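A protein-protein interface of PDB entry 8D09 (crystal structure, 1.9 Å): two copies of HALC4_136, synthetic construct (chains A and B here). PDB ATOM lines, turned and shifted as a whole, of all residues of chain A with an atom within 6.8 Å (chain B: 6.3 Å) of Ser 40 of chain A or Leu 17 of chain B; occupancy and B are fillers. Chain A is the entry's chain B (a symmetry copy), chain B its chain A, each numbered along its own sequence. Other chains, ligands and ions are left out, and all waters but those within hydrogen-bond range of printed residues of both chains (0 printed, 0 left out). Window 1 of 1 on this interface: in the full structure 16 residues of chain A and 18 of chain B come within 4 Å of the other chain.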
ATOM      1  N   ILE A  35      27.098  13.930 -24.161  1.00  0.00           N
ATOM      2  CA  ILE A  35      27.071  15.148 -23.332  1.00  0.00           C
ATOM      3  C   ILE A  35      26.594  14.799 -21.907  1.00  0.00           C
ATOM      4  O   ILE A  35      27.205  15.213 -20.894  1.00  0.00           O
ATOM      5  CB  ILE A  35      26.180  16.230 -23.994  1.00  0.00           C
ATOM      6  CG1 ILE A  35      26.883  16.709 -25.295  1.00  0.00           C
ATOM      7  CG2 ILE A  35      25.876  17.327 -23.029  1.00  0.00           C
ATOM      8  CD1 ILE A  35      26.001  17.586 -26.171  1.00  0.00           C
ATOM      9  N   ALA A  36      25.487  14.064 -21.790  1.00  0.00           N
ATOM     10  CA  ALA A  36      25.009  13.764 -20.423  1.00  0.00           C
ATOM     11  C   ALA A  36      26.060  12.988 -19.646  1.00  0.00           C
ATOM     12  O   ALA A  36      26.204  13.163 -18.416  1.00  0.00           O
ATOM     13  CB  ALA A  36      23.695  12.982 -20.445  1.00  0.00           C
ATOM     14  N   THR A  37      26.760  12.063 -20.313  1.00  0.00           N
ATOM     15  CA  THR A  37      27.712  11.218 -19.582  1.00  0.00           C
ATOM     16  C   THR A  37      28.883  12.060 -19.122  1.00  0.00           C
ATOM     17  O   THR A  37      29.338  11.921 -18.004  1.00  0.00           O
ATOM     18  CB  THR A  37      28.172  10.033 -20.436  1.00  0.00           C
ATOM     19  OG1 THR A  37      27.042   9.185 -20.655  1.00  0.00           O
ATOM     20  CG2 THR A  37      29.304   9.236 -19.773  1.00  0.00           C
ATOM     21  N   LEU A  38      29.348  12.985 -19.981  1.00  0.00           N
ATOM     22  CA  LEU A  38      30.338  13.986 -19.600  1.00  0.00           C
ATOM     23  C   LEU A  38      29.876  14.820 -18.418  1.00  0.00           C
ATOM     24  O   LEU A  38      30.685  15.123 -17.516  1.00  0.00           O
ATOM     25  CB  LEU A  38      30.627  14.867 -20.824  1.00  0.00           C
ATOM     26  CG  LEU A  38      31.530  14.197 -21.868  1.00  0.00           C
ATOM     27  CD1 LEU A  38      31.629  15.163 -23.053  1.00  0.00           C
ATOM     28  CD2 LEU A  38      32.941  13.951 -21.331  1.00  0.00           C
ATOM     29  N   ILE A  39      28.580  15.181 -18.356  1.00  0.00           N
ATOM     30  CA  ILE A  39      28.167  16.007 -17.201  1.00  0.00           C
ATOM     31  C   ILE A  39      28.219  15.190 -15.919  1.00  0.00           C
ATOM     32  O   ILE A  39      28.719  15.651 -14.851  1.00  0.00           O
ATOM     33  CB  ILE A  39      26.766  16.599 -17.394  1.00  0.00           C
ATOM     34  CG1 ILE A  39      26.800  17.523 -18.591  1.00  0.00           C
ATOM     35  CG2 ILE A  39      26.338  17.311 -16.102  1.00  0.00           C
ATOM     36  CD1 ILE A  39      25.408  18.036 -18.956  1.00  0.00           C
ATOM     37  N   SER A  40      27.709  13.937 -15.999  1.00  0.00           N
ATOM     38  CA  SER A  40      27.920  13.011 -14.870  1.00  0.00           C
ATOM     39  C   SER A  40      29.394  12.864 -14.477  1.00  0.00           C
ATOM     40  O   SER A  40      29.730  12.936 -13.285  1.00  0.00           O
ATOM     41  CB  SER A  40      27.330  11.661 -15.224  1.00  0.00           C
ATOM     42  OG  SER A  40      27.307  10.754 -14.138  1.00  0.00           O
ATOM     43  N   LEU A  41      30.298  12.622 -15.460  1.00  0.00           N
ATOM     44  CA  LEU A  41      31.720  12.511 -15.125  1.00  0.00           C
ATOM     45  C   LEU A  41      32.256  13.782 -14.470  1.00  0.00           C
ATOM     46  O   LEU A  41      33.045  13.716 -13.524  1.00  0.00           O
ATOM     47  CB  LEU A  41      32.556  12.174 -16.359  1.00  0.00           C
ATOM     48  CG  LEU A  41      32.563  10.719 -16.733  1.00  0.00           C
ATOM     49  CD1 LEU A  41      32.977  10.637 -18.182  1.00  0.00           C
ATOM     50  CD2 LEU A  41      33.524   9.941 -15.943  1.00  0.00           C
ATOM     51  N   LEU A  42      31.848  14.953 -14.949  1.00  0.00           N
ATOM     52  CA  LEU A  42      32.296  16.206 -14.334  1.00  0.00           C
ATOM     53  C   LEU A  42      31.901  16.264 -12.863  1.00  0.00           C
ATOM     54  O   LEU A  42      32.705  16.660 -11.993  1.00  0.00           O
ATOM     55  CB  LEU A  42      31.655  17.381 -15.072  1.00  0.00           C
ATOM     56  CG  LEU A  42      32.013  18.779 -14.663  1.00  0.00           C
ATOM     57  CD1 LEU A  42      33.527  18.906 -14.833  1.00  0.00           C
ATOM     58  CD2 LEU A  42      31.259  19.765 -15.515  1.00  0.00           C
ATOM     59  N   ALA A  43      30.686  15.815 -12.548  1.00  0.00           N
ATOM     60  CA  ALA A  43      30.271  15.799 -11.140  1.00  0.00           C
ATOM     61  C   ALA A  43      31.077  14.786 -10.345  1.00  0.00           C
ATOM     62  O   ALA A  43      31.514  15.045  -9.203  1.00  0.00           O
ATOM     63  CB  ALA A  43      28.782  15.469 -11.024  1.00  0.00           C
ATOM     64  N   LEU A  44      31.253  13.586 -10.897  1.00  0.00           N
ATOM     65  CA  LEU A  44      32.039  12.568 -10.179  1.00  0.00           C
ATOM     66  C   LEU A  44      33.474  13.031  -9.887  1.00  0.00           C
ATOM     67  O   LEU A  44      33.950  12.979  -8.728  1.00  0.00           O
ATOM     68  CB  LEU A  44      32.081  11.266 -10.988  1.00  0.00           C
ATOM     69  CG  LEU A  44      33.000  10.174 -10.497  1.00  0.00           C
ATOM     70  CD1 LEU A  44      32.737   9.791  -9.062  1.00  0.00           C
ATOM     71  CD2 LEU A  44      32.944   8.968 -11.418  1.00  0.00           C
ATOM     72  N   ILE A  45      34.174  13.518 -10.905  1.00  0.00           N
ATOM     73  CA  ILE A  45      35.536  14.012 -10.712  1.00  0.00           C
ATOM     74  C   ILE A  45      35.570  15.158  -9.705  1.00  0.00           C
ATOM     75  O   ILE A  45      36.525  15.312  -8.917  1.00  0.00           O
ATOM     76  CB  ILE A  45      36.113  14.493 -12.054  1.00  0.00           C
ATOM     77  CG1 ILE A  45      36.139  13.405 -13.130  1.00  0.00           C
ATOM     78  CG2 ILE A  45      37.507  15.019 -11.864  1.00  0.00           C
ATOM     79  CD1 ILE A  45      36.389  14.003 -14.525  1.00  0.00           C
ATOM     80  N   SER A  46      34.576  16.056  -9.790  1.00  0.00           N
ATOM     81  CA  SER A  46      34.527  17.167  -8.848  1.00  0.00           C
ATOM     82  C   SER A  46      34.369  16.675  -7.416  1.00  0.00           C
ATOM     83  O   SER A  46      35.029  17.181  -6.490  1.00  0.00           O
ATOM     84  CB  SER A  46      33.379  18.083  -9.236  1.00  0.00           C
ATOM     85  OG  SER A  46      33.728  18.809 -10.435  1.00  0.00           O
ATOM     86  N   ILE A  57      27.838  23.017 -12.409  1.00  0.00           N
ATOM     87  CA  ILE A  57      27.284  21.959 -13.273  1.00  0.00           C
ATOM     88  C   ILE A  57      25.997  22.405 -13.970  1.00  0.00           C
ATOM     89  O   ILE A  57      25.744  22.029 -15.119  1.00  0.00           O
ATOM     90  CB  ILE A  57      27.040  20.660 -12.479  1.00  0.00           C
ATOM     91  CG1 ILE A  57      28.226  20.336 -11.573  1.00  0.00           C
ATOM     92  CG2 ILE A  57      26.802  19.478 -13.432  1.00  0.00           C
ATOM     93  CD1 ILE A  57      29.469  20.008 -12.319  1.00  0.00           C
ATOM     94  N   TYR A  60      25.583  23.508 -17.866  1.00  0.00           N
ATOM     95  CA  TYR A  60      25.611  22.429 -18.848  1.00  0.00           C
ATOM     96  C   TYR A  60      24.317  21.653 -18.892  1.00  0.00           C
ATOM     97  O   TYR A  60      23.880  21.251 -19.979  1.00  0.00           O
ATOM     98  CB  TYR A  60      26.760  21.577 -18.462  1.00  0.00           C
ATOM     99  CG  TYR A  60      28.133  22.205 -18.622  1.00  0.00           C
ATOM    100  CD1 TYR A  60      28.581  22.728 -19.828  1.00  0.00           C
ATOM    101  CD2 TYR A  60      28.924  22.359 -17.513  1.00  0.00           C
ATOM    102  CE1 TYR A  60      29.870  23.258 -19.952  1.00  0.00           C
ATOM    103  CE2 TYR A  60      30.198  22.909 -17.609  1.00  0.00           C
ATOM    104  CZ  TYR A  60      30.668  23.345 -18.814  1.00  0.00           C
ATOM    105  OH  TYR A  60      31.936  23.907 -18.811  1.00  0.00           O
ATOM    106  N   ILE A  61      23.693  21.383 -17.737  1.00  0.00           N
ATOM    107  CA  ILE A  61      22.441  20.638 -17.747  1.00  0.00           C
ATOM    108  C   ILE A  61      21.389  21.440 -18.487  1.00  0.00           C
ATOM    109  O   ILE A  61      20.647  20.897 -19.314  1.00  0.00           O
ATOM    110  CB  ILE A  61      21.973  20.285 -16.325  1.00  0.00           C
ATOM    111  CG1 ILE A  61      22.991  19.364 -15.607  1.00  0.00           C
ATOM    112  CG2 ILE A  61      20.597  19.700 -16.324  1.00  0.00           C
ATOM    113  CD1 ILE A  61      22.582  19.109 -14.146  1.00  0.00           C
ATOM    114  N   LEU A  64      22.033  21.195 -22.230  1.00  0.00           N
ATOM    115  CA  LEU A  64      21.554  19.889 -22.694  1.00  0.00           C
ATOM    116  C   LEU A  64      20.027  19.885 -22.841  1.00  0.00           C
ATOM    117  O   LEU A  64      19.489  19.453 -23.880  1.00  0.00           O
ATOM    118  CB  LEU A  64      22.014  18.809 -21.720  1.00  0.00           C
ATOM    119  CG  LEU A  64      21.477  17.388 -21.898  1.00  0.00           C
ATOM    120  CD1 LEU A  64      21.723  16.893 -23.282  1.00  0.00           C
ATOM    121  CD2 LEU A  64      22.107  16.448 -20.832  1.00  0.00           C
ATOM    122  N   ALA B  10      26.250  14.286  -6.814  1.00  0.00           N
ATOM    123  CA  ALA B  10      26.517  13.683  -8.141  1.00  0.00           C
ATOM    124  C   ALA B  10      25.508  12.599  -8.501  1.00  0.00           C
ATOM    125  O   ALA B  10      25.152  12.398  -9.685  1.00  0.00           O
ATOM    126  CB  ALA B  10      27.932  13.157  -8.150  1.00  0.00           C
ATOM    127  N   GLU B  12      22.329  12.717  -7.543  1.00  0.00           N
ATOM    128  CA  GLU B  12      21.102  13.423  -7.941  1.00  0.00           C
ATOM    129  C   GLU B  12      21.193  13.988  -9.369  1.00  0.00           C
ATOM    130  O   GLU B  12      20.215  13.944 -10.179  1.00  0.00           O
ATOM    131  CB  GLU B  12      20.810  14.558  -6.955  1.00  0.00           C
ATOM    132  CG  GLU B  12      19.963  14.206  -5.726  1.00  0.00           C
ATOM    133  CD  GLU B  12      20.398  15.007  -4.496  1.00  0.00           C
ATOM    134  OE1 GLU B  12      20.911  16.144  -4.653  1.00  0.00           O
ATOM    135  OE2 GLU B  12      20.194  14.498  -3.376  1.00  0.00           O
ATOM    136  N   ILE B  13      22.357  14.514  -9.713  1.00  0.00           N
ATOM    137  CA  ILE B  13      22.615  15.006 -11.077  1.00  0.00           C
ATOM    138  C   ILE B  13      22.498  13.887 -12.097  1.00  0.00           C
ATOM    139  O   ILE B  13      21.822  14.020 -13.136  1.00  0.00           O
ATOM    140  CB  ILE B  13      24.022  15.620 -11.128  1.00  0.00           C
ATOM    141  CG1 ILE B  13      24.024  17.005 -10.534  1.00  0.00           C
ATOM    142  CG2 ILE B  13      24.627  15.816 -12.473  1.00  0.00           C
ATOM    143  CD1 ILE B  13      25.416  17.429 -10.054  1.00  0.00           C
ATOM    144  N   THR B  14      23.135  12.746 -11.822  1.00  0.00           N
ATOM    145  CA  THR B  14      23.092  11.623 -12.773  1.00  0.00           C
ATOM    146  C   THR B  14      21.652  11.101 -12.930  1.00  0.00           C
ATOM    147  O   THR B  14      21.201  10.745 -14.040  1.00  0.00           O
ATOM    148  CB  THR B  14      24.083  10.558 -12.272  1.00  0.00           C
ATOM    149  OG1 THR B  14      25.423  11.147 -12.165  1.00  0.00           O
ATOM    150  CG2 THR B  14      24.209   9.385 -13.236  1.00  0.00           C
ATOM    151  N   LYS B  15      20.876  11.040 -11.839  1.00  0.00           N
ATOM    152  CA  LYS B  15      19.482  10.599 -12.008  1.00  0.00           C
ATOM    153  C   LYS B  15      18.687  11.621 -12.810  1.00  0.00           C
ATOM    154  O   LYS B  15      17.803  11.264 -13.591  1.00  0.00           O
ATOM    155  CB  LYS B  15      18.785  10.361 -10.652  1.00  0.00           C
ATOM    156  CG  LYS B  15      19.491   9.317  -9.810  1.00  0.00           C
ATOM    157  CD  LYS B  15      18.630   8.967  -8.633  1.00  0.00           C
ATOM    158  CE  LYS B  15      19.010   7.666  -7.984  1.00  0.00           C
ATOM    159  NZ  LYS B  15      18.069   7.456  -6.804  1.00  0.00           N
ATOM    160  N   ARG B  16      18.952  12.906 -12.594  1.00  0.00           N
ATOM    161  CA  ARG B  16      18.304  13.935 -13.415  1.00  0.00           C
ATOM    162  C   ARG B  16      18.598  13.754 -14.895  1.00  0.00           C
ATOM    163  O   ARG B  16      17.690  13.847 -15.735  1.00  0.00           O
ATOM    164  CB  ARG B  16      18.774  15.300 -12.927  1.00  0.00           C
ATOM    165  CG  ARG B  16      18.108  16.455 -13.584  1.00  0.00           C
ATOM    166  CD  ARG B  16      18.526  17.686 -12.857  1.00  0.00           C
ATOM    167  NE  ARG B  16      18.147  18.905 -13.562  1.00  0.00           N
ATOM    168  CZ  ARG B  16      18.651  20.085 -13.250  1.00  0.00           C
ATOM    169  NH1 ARG B  16      19.569  20.187 -12.322  1.00  0.00           N
ATOM    170  NH2 ARG B  16      18.231  21.170 -13.906  1.00  0.00           N
ATOM    171  N   LEU B  17      19.862  13.478 -15.228  1.00  0.00           N
ATOM    172  CA  LEU B  17      20.235  13.256 -16.616  1.00  0.00           C
ATOM    173  C   LEU B  17      19.565  12.009 -17.183  1.00  0.00           C
ATOM    174  O   LEU B  17      19.110  12.006 -18.342  1.00  0.00           O
ATOM    175  CB  LEU B  17      21.745  13.157 -16.679  1.00  0.00           C
ATOM    176  CG  LEU B  17      22.482  14.485 -16.357  1.00  0.00           C
ATOM    177  CD1 LEU B  17      23.923  14.211 -16.035  1.00  0.00           C
ATOM    178  CD2 LEU B  17      22.191  15.480 -17.519  1.00  0.00           C
ATOM    179  N   LEU B  18      19.478  10.944 -16.384  1.00  0.00           N
ATOM    180  CA  LEU B  18      18.778   9.752 -16.869  1.00  0.00           C
ATOM    181  C   LEU B  18      17.294  10.078 -17.165  1.00  0.00           C
ATOM    182  O   LEU B  18      16.754   9.694 -18.218  1.00  0.00           O
ATOM    183  CB  LEU B  18      18.884   8.639 -15.854  1.00  0.00           C
ATOM    184  CG  LEU B  18      20.127   7.800 -15.761  1.00  0.00           C
ATOM    185  CD1 LEU B  18      20.199   7.284 -14.340  1.00  0.00           C
ATOM    186  CD2 LEU B  18      19.947   6.673 -16.714  1.00  0.00           C
ATOM    187  N   GLU B  19      16.628  10.823 -16.266  1.00  0.00           N
ATOM    188  CA  GLU B  19      15.220  11.177 -16.515  1.00  0.00           C
ATOM    189  C   GLU B  19      15.072  12.011 -17.769  1.00  0.00           C
ATOM    190  O   GLU B  19      14.051  11.889 -18.495  1.00  0.00           O
ATOM    191  CB  GLU B  19      14.610  11.882 -15.308  1.00  0.00           C
ATOM    192  CG  GLU B  19      14.786  11.070 -13.992  1.00  0.00           C
ATOM    193  CD  GLU B  19      13.849   9.840 -13.892  1.00  0.00           C
ATOM    194  OE1 GLU B  19      13.119   9.548 -14.875  1.00  0.00           O
ATOM    195  OE2 GLU B  19      13.898   9.114 -12.873  1.00  0.00           O
ATOM    196  N   LEU B  20      16.048  12.915 -18.022  1.00  0.00           N
ATOM    197  CA  LEU B  20      15.987  13.702 -19.253  1.00  0.00           C
ATOM    198  C   LEU B  20      16.042  12.786 -20.463  1.00  0.00           C
ATOM    199  O   LEU B  20      15.221  12.916 -21.397  1.00  0.00           O
ATOM    200  CB  LEU B  20      17.114  14.725 -19.327  1.00  0.00           C
ATOM    201  CG  LEU B  20      17.041  15.936 -18.395  1.00  0.00           C
ATOM    202  CD1 LEU B  20      18.317  16.749 -18.419  1.00  0.00           C
ATOM    203  CD2 LEU B  20      15.824  16.834 -18.774  1.00  0.00           C
ATOM    204  N   LEU B  21      17.035  11.891 -20.504  1.00  0.00           N
ATOM    205  CA  LEU B  21      17.186  11.064 -21.708  1.00  0.00           C
ATOM    206  C   LEU B  21      16.063  10.020 -21.841  1.00  0.00           C
ATOM    207  O   LEU B  21      15.837   9.496 -22.943  1.00  0.00           O
ATOM    208  CB  LEU B  21      18.517  10.305 -21.708  1.00  0.00           C
ATOM    209  CG  LEU B  21      19.797  11.085 -21.890  1.00  0.00           C
ATOM    210  CD1 LEU B  21      21.023  10.138 -21.829  1.00  0.00           C
ATOM    211  CD2 LEU B  21      19.796  11.796 -23.241  1.00  0.00           C
ATOM    212  N   LEU B  22      15.410   9.624 -20.736  1.00  0.00           N
ATOM    213  CA  LEU B  22      14.345   8.627 -20.845  1.00  0.00           C
ATOM    214  C   LEU B  22      12.963   9.243 -21.014  1.00  0.00           C
ATOM    215  O   LEU B  22      11.977   8.510 -21.185  1.00  0.00           O
ATOM    216  CB  LEU B  22      14.286   7.745 -19.599  1.00  0.00           C
ATOM    217  CG  LEU B  22      15.446   6.827 -19.418  1.00  0.00           C
ATOM    218  CD1 LEU B  22      15.652   6.294 -18.065  1.00  0.00           C
ATOM    219  CD2 LEU B  22      15.298   5.583 -20.368  1.00  0.00           C
ATOM    220  N   LEU B  38      25.262   6.071 -18.196  1.00  0.00           N
ATOM    221  CA  LEU B  38      24.764   6.765 -17.013  1.00  0.00           C
ATOM    222  C   LEU B  38      24.343   5.793 -15.924  1.00  0.00           C
ATOM    223  O   LEU B  38      24.600   6.055 -14.743  1.00  0.00           O
ATOM    224  CB  LEU B  38      23.541   7.636 -17.410  1.00  0.00           C
ATOM    225  CG  LEU B  38      23.837   8.962 -18.125  1.00  0.00           C
ATOM    226  CD1 LEU B  38      22.467   9.542 -18.571  1.00  0.00           C
ATOM    227  CD2 LEU B  38      24.577   9.958 -17.175  1.00  0.00           C
ATOM    228  N   LEU B  41      27.574   4.680 -14.348  1.00  0.00           N
ATOM    229  CA  LEU B  41      28.090   5.759 -13.493  1.00  0.00           C
ATOM    230  C   LEU B  41      27.311   5.919 -12.205  1.00  0.00           C
ATOM    231  O   LEU B  41      27.895   6.183 -11.152  1.00  0.00           O
ATOM    232  CB  LEU B  41      28.098   7.098 -14.219  1.00  0.00           C
ATOM    233  CG  LEU B  41      29.291   7.265 -15.145  1.00  0.00           C
ATOM    234  CD1 LEU B  41      28.996   8.353 -16.160  1.00  0.00           C
ATOM    235  CD2 LEU B  41      30.559   7.674 -14.424  1.00  0.00           C
ATOM    236  N   LEU B  42      25.989   5.859 -12.267  1.00  0.00           N
ATOM    237  CA  LEU B  42      25.166   5.894 -11.056  1.00  0.00           C
ATOM    238  C   LEU B  42      25.590   4.809 -10.082  1.00  0.00           C
ATOM    239  O   LEU B  42      25.763   5.057  -8.873  1.00  0.00           O
ATOM    240  CB  LEU B  42      23.694   5.712 -11.480  1.00  0.00           C
ATOM    241  CG  LEU B  42      22.617   5.646 -10.423  1.00  0.00           C
ATOM    242  CD1 LEU B  42      22.825   6.909  -9.654  1.00  0.00           C
ATOM    243  CD2 LEU B  42      21.270   5.642 -11.086  1.00  0.00           C
ATOM    244  N   ILE B  45      29.259   5.760  -8.714  1.00  0.00           N
ATOM    245  CA  ILE B  45      29.222   6.853  -7.761  1.00  0.00           C
ATOM    246  C   ILE B  45      28.588   6.385  -6.459  1.00  0.00           C
ATOM    247  O   ILE B  45      28.961   6.839  -5.365  1.00  0.00           O
ATOM    248  CB  ILE B  45      28.462   8.049  -8.350  1.00  0.00           C
ATOM    249  CG1 ILE B  45      29.051   8.507  -9.676  1.00  0.00           C
ATOM    250  CG2 ILE B  45      28.429   9.229  -7.342  1.00  0.00           C
ATOM    251  CD1 ILE B  45      28.103   9.397 -10.381  1.00  0.00           C
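Among the printed residues, merely in contact across the chains: Ala 36 of chain A with Leu 17 of chain B (3.5 Å), Ala 36 of chain A with Leu 38 of chain B (3.8 Å), Thr 37 of chain A with Leu 41 of chain B (3.7 Å), Ile 39 of chain A with Leu 17 of chain B (3.9 Å), Ser 40 of chain A with Leu 17 of chain B (3.8 Å), Ser 40 of chain A with Leu 38 of chain B (3.8 Å), Ser 40 of chain A with Leu 41 of chain B (3.6 Å), Ala 43 of chain A with Ala 10 of chain B (3.8 Å), Leu 44 of chain A with Ile 45 of chain B (3.95 Å), Ile 61 of chain A with Arg 16 of chain B (3.7 Å) and Leu 64 of chain A with Leu 17 of chain B (3.5 Å).
The backbone carbonyl oxygen (O) of Ala 10 of chain B lies within hydrogen-bond range of the side-chain hydroxyl (OG1) of Thr 14 of chain B (2.8 Å).
Of chain B, only Thr 14, Leu 17, Leu 38 and Leu 41 come within 4 Å of Ser 40 of chain A. Of chain A, only Ala 36, Ile 39, Ser 40 and Leu 64 come within 4 Å of Leu 17 of chain B. Printed residues of chain A within 4 Å of Arg 16 of chain B: Ile 61. Of the printed residues of chain A, Thr 14 of chain B touches Ser 40. Of the printed residues of chain A, Leu 38 of chain B touches Ala 36 and Ser 40. Glu 12 of chain B touches none of the printed residues of chain A. The nearest residue of chain A that does not touch Leu 17 of chain B is Ile 61 of chain A (4.4 Å).
Of the 16 printed residues of chain B, 7 touch a printed residue of chain A. Along chain B the printed residues that touch a printed residue of chain A span positions 10 to 45. Among the printed residues, 12 pairs touch across the chains. Among the printed residues, no Asp or Glu carboxylate lies within 4 Å of a Lys or Arg side-chain nitrogen of the other chain.
4 positions are printed for both chains.
The side-chain hydroxyl (OG1) of Thr 14 of chain B sits at hydrogen-bond distance from the side-chain hydroxyl (OG) of Ser 40 of chain A (2.8 Å).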
